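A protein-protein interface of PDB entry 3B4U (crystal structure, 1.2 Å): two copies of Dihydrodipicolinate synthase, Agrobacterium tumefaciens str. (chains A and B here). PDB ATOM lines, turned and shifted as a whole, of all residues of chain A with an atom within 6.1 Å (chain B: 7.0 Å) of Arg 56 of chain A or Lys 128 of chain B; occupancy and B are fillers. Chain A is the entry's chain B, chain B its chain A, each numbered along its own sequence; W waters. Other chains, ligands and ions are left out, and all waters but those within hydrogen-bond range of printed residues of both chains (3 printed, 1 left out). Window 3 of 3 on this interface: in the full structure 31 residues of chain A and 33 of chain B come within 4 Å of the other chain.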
ATOM      1  N   GLY A  54       5.101  17.563  25.261  1.00  0.00           N
ATOM      2  CA  GLY A  54       5.402  18.530  24.238  1.00  0.00           C
ATOM      3  C   GLY A  54       6.706  18.261  23.518  1.00  0.00           C
ATOM      4  O   GLY A  54       7.608  17.552  23.998  1.00  0.00           O
ATOM      5  N   SER A  55       6.834  18.897  22.364  1.00  0.00           N
ATOM      6  CA  SER A  55       8.022  18.779  21.548  1.00  0.00           C
ATOM      7  C   SER A  55       9.240  19.427  22.197  1.00  0.00           C
ATOM      8  O   SER A  55      10.368  19.009  21.914  1.00  0.00           O
ATOM      9  CB  SER A  55       7.791  19.386  20.148  1.00  0.00           C
ATOM     10  OG  SER A  55       6.839  18.595  19.454  1.00  0.00           O
ATOM     11  N   ARG A  56       9.049  20.453  23.038  1.00  0.00           N
ATOM     12  CA  ARG A  56      10.147  20.996  23.823  1.00  0.00           C
ATOM     13  C   ARG A  56      10.356  20.197  25.098  1.00  0.00           C
ATOM     14  O   ARG A  56      11.499  19.904  25.467  1.00  0.00           O
ATOM     15  CB  ARG A  56       9.917  22.485  24.143  1.00  0.00           C
ATOM     16  CG  ARG A  56       9.928  23.356  22.919  1.00  0.00           C
ATOM     17  CD  ARG A  56       9.716  24.808  23.240  1.00  0.00           C
ATOM     18  NE  ARG A  56       8.379  25.136  23.718  1.00  0.00           N
ATOM     19  CZ  ARG A  56       8.112  25.604  24.930  1.00  0.00           C
ATOM     20  NH1 ARG A  56       9.038  25.671  25.888  1.00  0.00           N
ATOM     21  NH2 ARG A  56       6.893  26.012  25.189  1.00  0.00           N
ATOM     22  N   GLU A  57       9.267  19.771  25.755  1.00  0.00           N
ATOM     23  CA  GLU A  57       9.404  18.969  26.946  1.00  0.00           C
ATOM     24  C   GLU A  57      10.216  17.704  26.711  1.00  0.00           C
ATOM     25  O   GLU A  57      11.076  17.345  27.521  1.00  0.00           O
ATOM     26  CB  GLU A  57       8.033  18.573  27.488  1.00  0.00           C
ATOM     27  CG  GLU A  57       7.278  19.665  28.162  1.00  0.00           C
ATOM     28  CD  GLU A  57       5.955  19.214  28.678  1.00  0.00           C
ATOM     29  OE1 GLU A  57       5.257  18.433  27.997  1.00  0.00           O
ATOM     30  OE2 GLU A  57       5.579  19.653  29.783  1.00  0.00           O
ATOM     31  N   ARG A  58       9.986  17.029  25.592  1.00  0.00           N
ATOM     32  CA  ARG A  58      10.704  15.781  25.357  1.00  0.00           C
ATOM     33  C   ARG A  58      12.202  16.026  25.200  1.00  0.00           C
ATOM     34  O   ARG A  58      12.998  15.161  25.544  1.00  0.00           O
ATOM     35  CB  ARG A  58      10.114  15.046  24.167  1.00  0.00           C
ATOM     36  CG  ARG A  58      10.239  15.695  22.834  1.00  0.00           C
ATOM     37  CD  ARG A  58       9.525  14.869  21.766  1.00  0.00           C
ATOM     38  NE  ARG A  58      10.291  13.672  21.394  1.00  0.00           N
ATOM     39  CZ  ARG A  58       9.820  12.430  21.385  1.00  0.00           C
ATOM     40  NH1 ARG A  58       8.603  12.105  21.791  1.00  0.00           N
ATOM     41  NH2 ARG A  58      10.624  11.471  20.984  1.00  0.00           N
ATOM     42  N   GLN A  59      12.567  17.175  24.626  1.00  0.00           N
ATOM     43  CA  GLN A  59      13.981  17.525  24.476  1.00  0.00           C
ATOM     44  C   GLN A  59      14.629  17.765  25.827  1.00  0.00           C
ATOM     45  O   GLN A  59      15.738  17.313  26.081  1.00  0.00           O
ATOM     46  CB  GLN A  59      14.115  18.734  23.547  1.00  0.00           C
ATOM     47  CG  GLN A  59      13.607  18.455  22.134  1.00  0.00           C
ATOM     48  CD  GLN A  59      13.545  19.678  21.241  1.00  0.00           C
ATOM     49  OE1 GLN A  59      13.168  20.769  21.651  1.00  0.00           O
ATOM     50  NE2 GLN A  59      13.843  19.463  19.994  1.00  0.00           N
ATOM     51  N   ALA A  60      13.935  18.466  26.707  1.00  0.00           N
ATOM     52  CA  ALA A  60      14.413  18.707  28.056  1.00  0.00           C
ATOM     53  C   ALA A  60      14.557  17.390  28.819  1.00  0.00           C
ATOM     54  O   ALA A  60      15.532  17.173  29.515  1.00  0.00           O
ATOM     55  CB  ALA A  60      13.479  19.669  28.780  1.00  0.00           C
ATOM     56  N   ILE A  61      13.572  16.503  28.696  1.00  0.00           N
ATOM     57  CA  ILE A  61      13.589  15.239  29.400  1.00  0.00           C
ATOM     58  C   ILE A  61      14.743  14.368  28.923  1.00  0.00           C
ATOM     59  O   ILE A  61      15.500  13.823  29.736  1.00  0.00           O
ATOM     60  CB  ILE A  61      12.233  14.536  29.257  1.00  0.00           C
ATOM     61  CG1 ILE A  61      11.151  15.306  30.027  1.00  0.00           C
ATOM     62  CG2 ILE A  61      12.316  13.091  29.766  1.00  0.00           C
ATOM     63  CD1 ILE A  61       9.725  14.948  29.606  1.00  0.00           C
ATOM     64  N   ILE B  84      -0.531  19.665  25.049  1.00  0.00           N
ATOM     65  CA  ILE B  84      -0.829  21.018  25.504  1.00  0.00           C
ATOM     66  C   ILE B  84       0.263  21.987  25.060  1.00  0.00           C
ATOM     67  O   ILE B  84      -0.041  23.084  24.553  1.00  0.00           O
ATOM     68  CB  ILE B  84      -1.006  21.032  27.037  1.00  0.00           C
ATOM     69  CG1 ILE B  84      -2.260  20.231  27.419  1.00  0.00           C
ATOM     70  CG2 ILE B  84      -1.042  22.453  27.580  1.00  0.00           C
ATOM     71  CD1 ILE B  84      -2.257  19.685  28.880  1.00  0.00           C
ATOM     72  N   GLU B  85       1.529  21.606  25.211  1.00  0.00           N
ATOM     73  CA  GLU B  85       2.617  22.520  24.883  1.00  0.00           C
ATOM     74  C   GLU B  85       2.611  22.857  23.419  1.00  0.00           C
ATOM     75  O   GLU B  85       2.760  24.027  23.044  1.00  0.00           O
ATOM     76  CB  GLU B  85       3.959  21.903  25.277  1.00  0.00           C
ATOM     77  CG  GLU B  85       5.147  22.801  25.014  1.00  0.00           C
ATOM     78  CD  GLU B  85       6.456  22.173  25.457  1.00  0.00           C
ATOM     79  OE1 GLU B  85       6.909  21.182  24.878  1.00  0.00           O
ATOM     80  OE2 GLU B  85       7.110  22.714  26.379  1.00  0.00           O
ATOM     81  N   ASP B  86       2.481  21.864  22.543  1.00  0.00           N
ATOM     82  CA  ASP B  86       2.520  22.187  21.126  1.00  0.00           C
ATOM     83  C   ASP B  86       1.266  22.932  20.674  1.00  0.00           C
ATOM     84  O   ASP B  86       1.368  23.823  19.849  1.00  0.00           O
ATOM     85  CB  ASP B  86       2.711  20.954  20.266  1.00  0.00           C
ATOM     86  CG  ASP B  86       4.060  20.346  20.389  1.00  0.00           C
ATOM     87  OD1 ASP B  86       4.859  20.680  21.307  1.00  0.00           O
ATOM     88  OD2 ASP B  86       4.391  19.551  19.468  1.00  0.00           O
ATOM     89  N   ALA B  88      -0.496  25.024  22.444  1.00  0.00           N
ATOM     90  CA  ALA B  88      -0.316  26.395  22.928  1.00  0.00           C
ATOM     91  C   ALA B  88       0.751  27.114  22.127  1.00  0.00           C
ATOM     92  O   ALA B  88       0.560  28.267  21.727  1.00  0.00           O
ATOM     93  CB  ALA B  88       0.020  26.410  24.394  1.00  0.00           C
ATOM     94  N   ASP B  89       1.864  26.464  21.823  1.00  0.00           N
ATOM     95  CA  ASP B  89       2.924  27.120  21.056  1.00  0.00           C
ATOM     96  C   ASP B  89       2.400  27.518  19.675  1.00  0.00           C
ATOM     97  O   ASP B  89       2.557  28.681  19.258  1.00  0.00           O
ATOM     98  CB  ASP B  89       4.138  26.210  20.887  1.00  0.00           C
ATOM     99  CG  ASP B  89       5.045  26.108  22.124  1.00  0.00           C
ATOM    100  OD1 ASP B  89       4.836  26.779  23.142  1.00  0.00           O
ATOM    101  OD2 ASP B  89       6.024  25.325  22.023  1.00  0.00           O
ATOM    102  N   ALA B  92      -0.382  30.299  19.995  1.00  0.00           N
ATOM    103  CA  ALA B  92       0.155  31.609  20.374  1.00  0.00           C
ATOM    104  C   ALA B  92       0.885  32.250  19.219  1.00  0.00           C
ATOM    105  O   ALA B  92       0.778  33.468  18.994  1.00  0.00           O
ATOM    106  CB  ALA B  92       1.062  31.486  21.580  1.00  0.00           C
ATOM    107  N   PHE B 122      -8.328  21.563  27.001  1.00  0.00           N
ATOM    108  CA  PHE B 122      -8.540  22.893  26.442  1.00  0.00           C
ATOM    109  C   PHE B 122      -8.193  23.971  27.455  1.00  0.00           C
ATOM    110  O   PHE B 122      -7.523  24.939  27.139  1.00  0.00           O
ATOM    111  CB  PHE B 122      -9.977  23.088  25.960  1.00  0.00           C
ATOM    112  CG  PHE B 122     -10.291  22.377  24.679  1.00  0.00           C
ATOM    113  CD1 PHE B 122      -9.760  22.820  23.497  1.00  0.00           C
ATOM    114  CD2 PHE B 122     -11.125  21.280  24.647  1.00  0.00           C
ATOM    115  CE1 PHE B 122     -10.023  22.175  22.290  1.00  0.00           C
ATOM    116  CE2 PHE B 122     -11.426  20.641  23.434  1.00  0.00           C
ATOM    117  CZ  PHE B 122     -10.859  21.104  22.260  1.00  0.00           C
ATOM    118  N   SER B 123      -8.645  23.813  28.701  1.00  0.00           N
ATOM    119  CA  SER B 123      -8.303  24.781  29.762  1.00  0.00           C
ATOM    120  C   SER B 123      -6.799  24.953  29.906  1.00  0.00           C
ATOM    121  O   SER B 123      -6.310  26.079  30.011  1.00  0.00           O
ATOM    122  CB  SER B 123      -8.879  24.332  31.082  1.00  0.00           C
ATOM    123  OG  SER B 123      -8.545  25.314  32.069  1.00  0.00           O
ATOM    124  N   ALA B 124      -6.052  23.846  29.876  1.00  0.00           N
ATOM    125  CA  ALA B 124      -4.605  23.910  30.022  1.00  0.00           C
ATOM    126  C   ALA B 124      -3.953  24.595  28.834  1.00  0.00           C
ATOM    127  O   ALA B 124      -3.012  25.362  28.997  1.00  0.00           O
ATOM    128  CB  ALA B 124      -4.025  22.493  30.241  1.00  0.00           C
ATOM    129  N   VAL B 125      -4.456  24.336  27.629  1.00  0.00           N
ATOM    130  CA  VAL B 125      -3.963  25.034  26.465  1.00  0.00           C
ATOM    131  C   VAL B 125      -4.159  26.541  26.627  1.00  0.00           C
ATOM    132  O   VAL B 125      -3.247  27.338  26.361  1.00  0.00           O
ATOM    133  CB  VAL B 125      -4.608  24.499  25.158  1.00  0.00           C
ATOM    134  CG1 VAL B 125      -4.216  25.363  23.981  1.00  0.00           C
ATOM    135  CG2 VAL B 125      -4.188  23.050  24.923  1.00  0.00           C
ATOM    136  N   PHE B 126      -5.364  26.945  27.009  1.00  0.00           N
ATOM    137  CA  PHE B 126      -5.675  28.371  27.083  1.00  0.00           C
ATOM    138  C   PHE B 126      -4.844  29.059  28.173  1.00  0.00           C
ATOM    139  O   PHE B 126      -4.317  30.164  27.955  1.00  0.00           O
ATOM    140  CB  PHE B 126      -7.142  28.596  27.340  1.00  0.00           C
ATOM    141  CG  PHE B 126      -8.063  27.952  26.323  1.00  0.00           C
ATOM    142  CD1 PHE B 126      -7.653  27.670  25.020  1.00  0.00           C
ATOM    143  CD2 PHE B 126      -9.346  27.577  26.701  1.00  0.00           C
ATOM    144  CE1 PHE B 126      -8.486  27.062  24.131  1.00  0.00           C
ATOM    145  CE2 PHE B 126     -10.192  26.957  25.788  1.00  0.00           C
ATOM    146  CZ  PHE B 126      -9.748  26.702  24.506  1.00  0.00           C
ATOM    147  N   SER B 127      -4.663  28.384  29.304  1.00  0.00           N
ATOM    148  CA  SER B 127      -3.818  28.931  30.379  1.00  0.00           C
ATOM    149  C   SER B 127      -2.380  29.100  29.885  1.00  0.00           C
ATOM    150  O   SER B 127      -1.701  30.074  30.214  1.00  0.00           O
ATOM    151  CB  SER B 127      -3.885  27.985  31.559  1.00  0.00           C
ATOM    152  OG  SER B 127      -3.209  26.804  31.285  1.00  0.00           O
ATOM    153  N   LYS B 128      -1.877  28.128  29.125  1.00  0.00           N
ATOM    154  CA  LYS B 128      -0.511  28.187  28.626  1.00  0.00           C
ATOM    155  C   LYS B 128      -0.322  29.286  27.575  1.00  0.00           C
ATOM    156  O   LYS B 128       0.711  29.971  27.529  1.00  0.00           O
ATOM    157  CB  LYS B 128      -0.102  26.828  28.060  1.00  0.00           C
ATOM    158  CG  LYS B 128       1.352  26.706  27.784  1.00  0.00           C
ATOM    159  CD  LYS B 128       2.120  26.603  29.068  1.00  0.00           C
ATOM    160  CE  LYS B 128       3.593  26.799  28.802  1.00  0.00           C
ATOM    161  NZ  LYS B 128       4.083  25.760  27.871  1.00  0.00           N
ATOM    162  N   ILE B 129      -1.305  29.495  26.715  1.00  0.00           N
ATOM    163  CA  ILE B 129      -1.260  30.642  25.816  1.00  0.00           C
ATOM    164  C   ILE B 129      -1.211  31.930  26.614  1.00  0.00           C
ATOM    165  O   ILE B 129      -0.419  32.832  26.295  1.00  0.00           O
ATOM    166  CB  ILE B 129      -2.460  30.672  24.861  1.00  0.00           C
ATOM    167  CG1 ILE B 129      -2.446  29.446  23.907  1.00  0.00           C
ATOM    168  CG2 ILE B 129      -2.443  31.977  24.071  1.00  0.00           C
ATOM    169  CD1 ILE B 129      -3.763  29.225  23.209  1.00  0.00           C
ATOM    170  N   GLY B 130      -2.040  32.020  27.640  1.00  0.00           N
ATOM    171  CA  GLY B 130      -2.065  33.167  28.528  1.00  0.00           C
ATOM    172  C   GLY B 130      -3.046  34.218  28.068  1.00  0.00           C
ATOM    173  O   GLY B 130      -4.010  33.935  27.356  1.00  0.00           O
ATOM    174  N   LYS B 131      -2.799  35.457  28.491  1.00  0.00           N
ATOM    175  CA  LYS B 131      -3.765  36.536  28.318  1.00  0.00           C
ATOM    176  C   LYS B 131      -4.040  36.860  26.854  1.00  0.00           C
ATOM    177  O   LYS B 131      -5.081  37.421  26.530  1.00  0.00           O
ATOM    178  CB  LYS B 131      -3.297  37.796  29.066  1.00  0.00           C
ATOM    179  CG  LYS B 131      -2.106  38.489  28.443  1.00  0.00           C
ATOM    180  CD  LYS B 131      -1.705  39.793  29.195  1.00  0.00           C
ATOM    181  CE  LYS B 131      -0.636  40.529  28.404  1.00  0.00           C
ATOM    182  NZ  LYS B 131      -0.069  41.744  29.077  1.00  0.00           N
HETATM  183  O   HOH W   1       2.382  19.289  26.695  1.00  0.00           O
HETATM  184  O   HOH W   2       9.784  22.328  27.540  1.00  0.00           O
HETATM  185  O   HOH W   3       6.475  24.444  28.234  1.00  0.00           O
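The side-chain carboxylate of Glu 85 of chain B is in hydrogen-bond range of the backbone NH of Ser 55 of chain A (3.4 Å). The guanidinium group (NH2) of Arg 56 of chain A is in salt-bridge range of the side-chain carboxylate (OE2) of Glu 85 of chain B (3.5 Å). The side-chain carboxylate (OE1) of Glu 85 of chain B lies within hydrogen-bond range of the backbone NH (N) of Glu 57 of chain A (2.9 Å). OG of Ser 55 of chain A sits at hydrogen-bond distance from OD2 of Asp 86 of chain B, at 2.6 Å. The side-chain carboxylate of Asp 89 of chain B lies within salt-bridge range of the guanidinium group of Arg 56 of chain A (2.9 Å).
Among the printed residues, pairs that only touch across the chains: Gly 54 of chain A with Glu 85 of chain B (3.1 Å), Gly 54 of chain A with Asp 86 of chain B (3.7 Å) and Arg 56 of chain A with Lys 128 of chain B (3.9 Å).
The backbone NH (N) of Gly 54 of chain A sits at hydrogen-bond distance from the side-chain carboxylate (OE1) of Glu 57 of chain A (2.9 Å). The backbone carbonyl oxygen of Ser 55 of chain A lies close to the side-chain amide oxygen of Gln 59 of chain A.
Of the 8 printed residues of chain A, 4 touch a printed residue of chain B.
No position is printed for both chains. Of the 8 pairs that touch across the chains among the printed residues, none has its exchanged pair printed and touching as well.
Water W3 lies within hydrogen-bond range of OE2 of Glu 85 of chain B (2.6 Å), NZ of Lys 128 of chain B (2.8 Å) and NH2 of Arg 56 of chain A (3.5 Å). Water W1 lies within hydrogen-bond range of the backbone NH of Glu 85 of chain B, the side-chain carboxylate of Glu 57 of chain A and the backbone NH of Ile 84 of chain B. Water W2 lies within hydrogen-bond range of OE2 of Glu 85 of chain B (2.9 Å) and N of Glu 57 of chain A (3.2 Å).
Printed residues of chain B within 4 Å of Gly 54 of chain A: Glu 85 (3.1 Å) and Asp 86 (3.7 Å). Printed residues of chain B within 4 Å of Ser 55 of chain A: Glu 85 (3.4 Å) and Asp 86 (2.6 Å). Printed residues of chain B within 4 Å of Glu 57 of chain A: Glu 85 (2.9 Å). Of the printed residues of chain A, Glu 85 of chain B touches Gly 54, Ser 55, Arg 56 and Glu 57. Printed residues of chain A within 4 Å of Asp 86 of chain B: Gly 54 (3.7 Å) and Ser 55 (2.6 Å). Of chain A, only Arg 56 comes within 4 Å of Lys 128 of chain B. The nearest residue of chain B that does not touch Arg 56 of chain A is Asp 86 of chain B (4.5 Å).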
